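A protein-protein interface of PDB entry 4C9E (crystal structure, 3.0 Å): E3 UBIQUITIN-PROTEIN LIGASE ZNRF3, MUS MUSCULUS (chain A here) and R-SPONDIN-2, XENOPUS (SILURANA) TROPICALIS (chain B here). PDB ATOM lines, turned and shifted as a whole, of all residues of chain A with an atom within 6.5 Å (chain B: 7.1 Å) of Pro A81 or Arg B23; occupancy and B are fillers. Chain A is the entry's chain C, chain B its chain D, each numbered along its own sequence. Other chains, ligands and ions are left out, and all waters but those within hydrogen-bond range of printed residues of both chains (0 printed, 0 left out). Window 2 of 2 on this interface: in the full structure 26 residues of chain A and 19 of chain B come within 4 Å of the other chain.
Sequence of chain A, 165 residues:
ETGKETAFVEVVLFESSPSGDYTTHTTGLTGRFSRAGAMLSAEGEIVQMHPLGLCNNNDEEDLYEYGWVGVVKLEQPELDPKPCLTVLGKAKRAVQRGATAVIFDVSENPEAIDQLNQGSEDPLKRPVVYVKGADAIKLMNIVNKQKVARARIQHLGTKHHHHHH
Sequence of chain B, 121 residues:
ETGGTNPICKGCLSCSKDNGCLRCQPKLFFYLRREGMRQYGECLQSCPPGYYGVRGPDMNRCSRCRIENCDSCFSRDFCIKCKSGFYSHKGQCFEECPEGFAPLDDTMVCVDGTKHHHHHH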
ATOM      1  N   LEU A  52       6.374 -33.687 -21.646  1.00  0.00           N
ATOM      2  CA  LEU A  52       5.021 -33.169 -21.788  1.00  0.00           C
ATOM      3  C   LEU A  52       3.995 -34.252 -22.142  1.00  0.00           C
ATOM      4  O   LEU A  52       2.805 -34.007 -22.068  1.00  0.00           O
ATOM      5  CB  LEU A  52       4.978 -32.035 -22.817  1.00  0.00           C
ATOM      6  CG  LEU A  52       5.508 -30.673 -22.350  1.00  0.00           C
ATOM      7  CD1 LEU A  52       7.012 -30.673 -22.088  1.00  0.00           C
ATOM      8  CD2 LEU A  52       5.149 -29.603 -23.371  1.00  0.00           C
ATOM      9  N   PRO A  77      13.647 -25.887 -17.577  1.00  0.00           N
ATOM     10  CA  PRO A  77      12.327 -25.696 -16.928  1.00  0.00           C
ATOM     11  C   PRO A  77      11.588 -24.421 -17.304  1.00  0.00           C
ATOM     12  O   PRO A  77      10.443 -24.234 -16.892  1.00  0.00           O
ATOM     13  CB  PRO A  77      12.654 -25.671 -15.429  1.00  0.00           C
ATOM     14  CG  PRO A  77      14.120 -25.425 -15.336  1.00  0.00           C
ATOM     15  CD  PRO A  77      14.753 -25.911 -16.603  1.00  0.00           C
ATOM     16  N   GLU A  78      12.264 -23.557 -18.057  1.00  0.00           N
ATOM     17  CA  GLU A  78      11.712 -22.306 -18.545  1.00  0.00           C
ATOM     18  C   GLU A  78      10.884 -22.586 -19.791  1.00  0.00           C
ATOM     19  O   GLU A  78      10.001 -21.806 -20.155  1.00  0.00           O
ATOM     20  CB  GLU A  78      12.854 -21.328 -18.861  1.00  0.00           C
ATOM     21  CG  GLU A  78      13.738 -20.944 -17.660  1.00  0.00           C
ATOM     22  CD  GLU A  78      14.910 -21.902 -17.357  1.00  0.00           C
ATOM     23  OE1 GLU A  78      15.137 -22.895 -18.077  1.00  0.00           O
ATOM     24  OE2 GLU A  78      15.626 -21.660 -16.366  1.00  0.00           O
ATOM     25  N   LEU A  79      11.166 -23.719 -20.432  1.00  0.00           N
ATOM     26  CA  LEU A  79      10.456 -24.118 -21.637  1.00  0.00           C
ATOM     27  C   LEU A  79       9.051 -24.614 -21.332  1.00  0.00           C
ATOM     28  O   LEU A  79       8.198 -24.609 -22.213  1.00  0.00           O
ATOM     29  CB  LEU A  79      11.253 -25.178 -22.379  1.00  0.00           C
ATOM     30  CG  LEU A  79      12.588 -24.633 -22.888  1.00  0.00           C
ATOM     31  CD1 LEU A  79      13.663 -25.712 -22.937  1.00  0.00           C
ATOM     32  CD2 LEU A  79      12.386 -23.991 -24.255  1.00  0.00           C
ATOM     33  N   ASP A  80       8.821 -25.071 -20.100  1.00  0.00           N
ATOM     34  CA  ASP A  80       7.458 -25.206 -19.569  1.00  0.00           C
ATOM     35  C   ASP A  80       7.370 -24.487 -18.217  1.00  0.00           C
ATOM     36  O   ASP A  80       7.784 -25.031 -17.188  1.00  0.00           O
ATOM     37  CB  ASP A  80       7.019 -26.668 -19.443  1.00  0.00           C
ATOM     38  CG  ASP A  80       5.515 -26.806 -19.237  1.00  0.00           C
ATOM     39  OD1 ASP A  80       4.911 -25.892 -18.630  1.00  0.00           O
ATOM     40  OD2 ASP A  80       4.932 -27.819 -19.683  1.00  0.00           O
ATOM     41  N   PRO A  81       6.831 -23.257 -18.219  1.00  0.00           N
ATOM     42  CA  PRO A  81       6.828 -22.453 -17.009  1.00  0.00           C
ATOM     43  C   PRO A  81       6.031 -23.118 -15.899  1.00  0.00           C
ATOM     44  O   PRO A  81       6.552 -23.317 -14.798  1.00  0.00           O
ATOM     45  CB  PRO A  81       6.159 -21.144 -17.454  1.00  0.00           C
ATOM     46  CG  PRO A  81       6.259 -21.134 -18.940  1.00  0.00           C
ATOM     47  CD  PRO A  81       6.152 -22.570 -19.329  1.00  0.00           C
ATOM     48  N   LYS A  82       4.786 -23.470 -16.201  1.00  0.00           N
ATOM     49  CA  LYS A  82       3.911 -24.110 -15.222  1.00  0.00           C
ATOM     50  C   LYS A  82       3.541 -25.519 -15.681  1.00  0.00           C
ATOM     51  O   LYS A  82       2.546 -25.722 -16.392  1.00  0.00           O
ATOM     52  CB  LYS A  82       2.681 -23.238 -14.932  1.00  0.00           C
ATOM     53  CG  LYS A  82       2.875 -22.325 -13.721  1.00  0.00           C
ATOM     54  CD  LYS A  82       2.732 -20.852 -14.068  1.00  0.00           C
ATOM     55  CE  LYS A  82       3.713 -20.021 -13.268  1.00  0.00           C
ATOM     56  NZ  LYS A  82       3.755 -18.618 -13.752  1.00  0.00           N
ATOM     57  N   PRO A  83       4.350 -26.503 -15.256  1.00  0.00           N
ATOM     58  CA  PRO A  83       4.202 -27.861 -15.757  1.00  0.00           C
ATOM     59  C   PRO A  83       2.851 -28.479 -15.435  1.00  0.00           C
ATOM     60  O   PRO A  83       2.159 -28.041 -14.508  1.00  0.00           O
ATOM     61  CB  PRO A  83       5.330 -28.628 -15.050  1.00  0.00           C
ATOM     62  CG  PRO A  83       5.626 -27.836 -13.826  1.00  0.00           C
ATOM     63  CD  PRO A  83       5.394 -26.409 -14.218  1.00  0.00           C
ATOM     64  N   LYS B  10       9.506 -28.335 -37.325  1.00  0.00           N
ATOM     65  CA  LYS B  10       8.641 -27.269 -37.864  1.00  0.00           C
ATOM     66  C   LYS B  10       7.359 -26.985 -37.078  1.00  0.00           C
ATOM     67  O   LYS B  10       6.797 -27.876 -36.426  1.00  0.00           O
ATOM     68  CB  LYS B  10       8.253 -27.604 -39.315  1.00  0.00           C
ATOM     69  CG  LYS B  10       7.298 -28.797 -39.488  1.00  0.00           C
ATOM     70  CD  LYS B  10       7.224 -29.292 -40.937  1.00  0.00           C
ATOM     71  CE  LYS B  10       8.212 -30.423 -41.236  1.00  0.00           C
ATOM     72  NZ  LYS B  10       7.619 -31.776 -41.068  1.00  0.00           N
ATOM     73  N   GLY B  11       6.888 -25.741 -37.213  1.00  0.00           N
ATOM     74  CA  GLY B  11       5.751 -25.206 -36.453  1.00  0.00           C
ATOM     75  C   GLY B  11       6.200 -24.843 -35.055  1.00  0.00           C
ATOM     76  O   GLY B  11       5.395 -24.600 -34.167  1.00  0.00           O
ATOM     77  N   CYS B  12       7.510 -24.756 -34.889  1.00  0.00           N
ATOM     78  CA  CYS B  12       8.132 -25.028 -33.624  1.00  0.00           C
ATOM     79  C   CYS B  12       8.727 -23.752 -33.052  1.00  0.00           C
ATOM     80  O   CYS B  12       9.514 -23.077 -33.713  1.00  0.00           O
ATOM     81  CB  CYS B  12       9.208 -26.090 -33.861  1.00  0.00           C
ATOM     82  SG  CYS B  12       9.330 -27.370 -32.588  1.00  0.00           S
ATOM     83  N   LEU B  13       8.318 -23.406 -31.837  1.00  0.00           N
ATOM     84  CA  LEU B  13       8.948 -22.310 -31.116  1.00  0.00           C
ATOM     85  C   LEU B  13      10.219 -22.860 -30.511  1.00  0.00           C
ATOM     86  O   LEU B  13      11.313 -22.422 -30.848  1.00  0.00           O
ATOM     87  CB  LEU B  13       8.043 -21.756 -30.009  1.00  0.00           C
ATOM     88  CG  LEU B  13       6.723 -21.070 -30.379  1.00  0.00           C
ATOM     89  CD1 LEU B  13       6.015 -20.644 -29.101  1.00  0.00           C
ATOM     90  CD2 LEU B  13       6.923 -19.881 -31.309  1.00  0.00           C
ATOM     91  N   SER B  14      10.057 -23.843 -29.630  1.00  0.00           N
ATOM     92  CA  SER B  14      11.178 -24.497 -28.973  1.00  0.00           C
ATOM     93  C   SER B  14      11.347 -25.883 -29.581  1.00  0.00           C
ATOM     94  O   SER B  14      10.361 -26.586 -29.799  1.00  0.00           O
ATOM     95  CB  SER B  14      10.909 -24.596 -27.480  1.00  0.00           C
ATOM     96  OG  SER B  14      10.379 -23.377 -26.983  1.00  0.00           O
ATOM     97  N   CYS B  15      12.599 -26.263 -29.838  1.00  0.00           N
ATOM     98  CA  CYS B  15      12.942 -27.408 -30.686  1.00  0.00           C
ATOM     99  C   CYS B  15      14.203 -28.086 -30.161  1.00  0.00           C
ATOM    100  O   CYS B  15      15.251 -27.446 -30.054  1.00  0.00           O
ATOM    101  CB  CYS B  15      13.182 -26.914 -32.121  1.00  0.00           C
ATOM    102  SG  CYS B  15      14.017 -28.050 -33.267  1.00  0.00           S
ATOM    103  N   GLY B  20      12.078 -33.132 -30.155  1.00  0.00           N
ATOM    104  CA  GLY B  20      11.345 -32.343 -31.146  1.00  0.00           C
ATOM    105  C   GLY B  20      10.682 -31.146 -30.493  1.00  0.00           C
ATOM    106  O   GLY B  20      11.263 -30.527 -29.598  1.00  0.00           O
ATOM    107  N   CYS B  21       9.455 -30.841 -30.908  1.00  0.00           N
ATOM    108  CA  CYS B  21       8.747 -29.648 -30.419  1.00  0.00           C
ATOM    109  C   CYS B  21       8.399 -29.690 -28.914  1.00  0.00           C
ATOM    110  O   CYS B  21       7.846 -30.671 -28.429  1.00  0.00           O
ATOM    111  CB  CYS B  21       7.483 -29.374 -31.266  1.00  0.00           C
ATOM    112  SG  CYS B  21       7.806 -28.707 -32.930  1.00  0.00           S
ATOM    113  N   LEU B  22       8.758 -28.619 -28.196  1.00  0.00           N
ATOM    114  CA  LEU B  22       8.403 -28.412 -26.776  1.00  0.00           C
ATOM    115  C   LEU B  22       7.307 -27.350 -26.580  1.00  0.00           C
ATOM    116  O   LEU B  22       6.567 -27.372 -25.587  1.00  0.00           O
ATOM    117  CB  LEU B  22       9.630 -27.980 -25.979  1.00  0.00           C
ATOM    118  CG  LEU B  22      10.901 -28.816 -26.109  1.00  0.00           C
ATOM    119  CD1 LEU B  22      12.033 -28.161 -25.329  1.00  0.00           C
ATOM    120  CD2 LEU B  22      10.677 -30.240 -25.628  1.00  0.00           C
ATOM    121  N   ARG B  23       7.246 -26.399 -27.510  1.00  0.00           N
ATOM    122  CA  ARG B  23       6.137 -25.453 -27.600  1.00  0.00           C
ATOM    123  C   ARG B  23       5.842 -25.113 -29.063  1.00  0.00           C
ATOM    124  O   ARG B  23       6.724 -25.219 -29.932  1.00  0.00           O
ATOM    125  CB  ARG B  23       6.426 -24.188 -26.781  1.00  0.00           C
ATOM    126  CG  ARG B  23       5.804 -24.211 -25.388  1.00  0.00           C
ATOM    127  CD  ARG B  23       6.554 -23.360 -24.367  1.00  0.00           C
ATOM    128  NE  ARG B  23       6.188 -21.940 -24.385  1.00  0.00           N
ATOM    129  CZ  ARG B  23       6.504 -21.058 -23.432  1.00  0.00           C
ATOM    130  NH1 ARG B  23       7.204 -21.424 -22.361  1.00  0.00           N
ATOM    131  NH2 ARG B  23       6.112 -19.794 -23.546  1.00  0.00           N
ATOM    132  N   CYS B  24       4.591 -24.716 -29.304  1.00  0.00           N
ATOM    133  CA  CYS B  24       4.058 -24.460 -30.644  1.00  0.00           C
ATOM    134  C   CYS B  24       3.913 -22.981 -30.980  1.00  0.00           C
ATOM    135  O   CYS B  24       3.727 -22.142 -30.096  1.00  0.00           O
ATOM    136  CB  CYS B  24       2.679 -25.116 -30.781  1.00  0.00           C
ATOM    137  SG  CYS B  24       2.739 -26.880 -31.136  1.00  0.00           S
ATOM    138  N   GLN B  25       3.990 -22.666 -32.269  1.00  0.00           N
ATOM    139  CA  GLN B  25       3.497 -21.381 -32.741  1.00  0.00           C
ATOM    140  C   GLN B  25       1.976 -21.403 -32.497  1.00  0.00           C
ATOM    141  O   GLN B  25       1.323 -22.406 -32.779  1.00  0.00           O
ATOM    142  CB  GLN B  25       3.842 -21.159 -34.212  1.00  0.00           C
ATOM    143  CG  GLN B  25       5.317 -20.862 -34.456  1.00  0.00           C
ATOM    144  CD  GLN B  25       5.765 -21.207 -35.869  1.00  0.00           C
ATOM    145  OE1 GLN B  25       4.974 -21.678 -36.688  1.00  0.00           O
ATOM    146  NE2 GLN B  25       7.044 -20.986 -36.159  1.00  0.00           N
ATOM    147  N   PHE B  30      -0.411 -29.029 -30.824  1.00  0.00           N
ATOM    148  CA  PHE B  30       0.687 -29.896 -30.373  1.00  0.00           C
ATOM    149  C   PHE B  30       0.345 -31.399 -30.424  1.00  0.00           C
ATOM    150  O   PHE B  30      -0.768 -31.805 -30.073  1.00  0.00           O
ATOM    151  CB  PHE B  30       1.090 -29.515 -28.953  1.00  0.00           C
ATOM    152  CG  PHE B  30       2.275 -30.255 -28.455  1.00  0.00           C
ATOM    153  CD1 PHE B  30       3.523 -29.983 -28.959  1.00  0.00           C
ATOM    154  CD2 PHE B  30       2.142 -31.225 -27.489  1.00  0.00           C
ATOM    155  CE1 PHE B  30       4.642 -30.664 -28.502  1.00  0.00           C
ATOM    156  CE2 PHE B  30       3.256 -31.907 -27.013  1.00  0.00           C
ATOM    157  CZ  PHE B  30       4.512 -31.631 -27.524  1.00  0.00           C
ATOM    158  N   CYS B  43       4.235 -29.741 -34.198  1.00  0.00           N
ATOM    159  CA  CYS B  43       3.233 -28.672 -34.147  1.00  0.00           C
ATOM    160  C   CYS B  43       2.442 -28.610 -35.453  1.00  0.00           C
ATOM    161  O   CYS B  43       2.980 -28.247 -36.491  1.00  0.00           O
ATOM    162  CB  CYS B  43       3.920 -27.339 -33.890  1.00  0.00           C
ATOM    163  SG  CYS B  43       4.490 -27.130 -32.190  1.00  0.00           S
ATOM    164  N   ASP B  58      -3.002 -23.597 -21.972  1.00  0.00           N
ATOM    165  CA  ASP B  58      -1.563 -23.808 -21.932  1.00  0.00           C
ATOM    166  C   ASP B  58      -1.041 -23.796 -23.356  1.00  0.00           C
ATOM    167  O   ASP B  58      -0.156 -23.009 -23.694  1.00  0.00           O
ATOM    168  CB  ASP B  58      -1.242 -25.150 -21.262  1.00  0.00           C
ATOM    169  CG  ASP B  58      -1.960 -25.325 -19.934  1.00  0.00           C
ATOM    170  OD1 ASP B  58      -2.045 -24.338 -19.178  1.00  0.00           O
ATOM    171  OD2 ASP B  58      -2.446 -26.440 -19.652  1.00  0.00           O
ATOM    172  N   MET B  59      -1.622 -24.665 -24.183  1.00  0.00           N
ATOM    173  CA  MET B  59      -1.270 -24.793 -25.596  1.00  0.00           C
ATOM    174  C   MET B  59      -2.495 -25.322 -26.339  1.00  0.00           C
ATOM    175  O   MET B  59      -3.505 -25.644 -25.714  1.00  0.00           O
ATOM    176  CB  MET B  59      -0.083 -25.753 -25.746  1.00  0.00           C
ATOM    177  CG  MET B  59      -0.403 -27.210 -25.417  1.00  0.00           C
ATOM    178  SD  MET B  59       0.913 -28.149 -24.597  1.00  0.00           S
ATOM    179  CE  MET B  59       2.364 -27.674 -25.541  1.00  0.00           C
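Pro A81 touches one residue of chain B. Of chain A, only Glu A78 (3.6 Å), Leu A79 (3.0 Å) and Pro A81 (3.4 Å) come within 4 Å of Arg B23. Printed residues of chain A within 4 Å of Leu B22: Leu A52 (3.4 Å) and Leu A79 (3.8 Å). Printed residues of chain B within 4 Å of Leu A52: Leu B22. Lys A82 touches none of the printed residues of chain B.
Among the printed residues, merely in contact across the chains: Leu A52 with Leu B22 (3.4 Å), Glu A78 with Arg B23 (3.6 Å), Leu A79 with Ser B14 (3.4 Å), Leu A79 with Leu B22 (3.8 Å) and Pro A81 with Arg B23 (3.4 Å).
The side-chain sulfur of Cys B12 forms a disulfide with the side-chain sulfur of Cys B21. The backbone NH (N) of Leu B13 is in hydrogen-bond range of the backbone carbonyl oxygen (O) of Arg B23 (3.1 Å). SG of Cys B24 is disulfide-bonded to SG of Cys B43 (2.1 Å). O of Ser B14 lies within hydrogen-bond range of N of Leu B22 (3.0 Å).
Of the 16 printed residues of chain B, 3 touch a printed residue of chain A. Hydrophobic or aromatic side chains of chain B within 4 Å of the printed part of chain A: Leu B22. Of the 8 printed residues of chain A, 4 touch a printed residue of chain B. Hydrophobic or aromatic side chains of chain A within 4 Å of the printed part of chain B: Leu A52, Leu A79 and Pro A81. Among the printed residues, no Asp or Glu carboxylate lies within 4 Å of a Lys or Arg side-chain nitrogen of the other chain.
NH1 of Arg B23 sits close to O of Leu A79 (3.3 Å).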
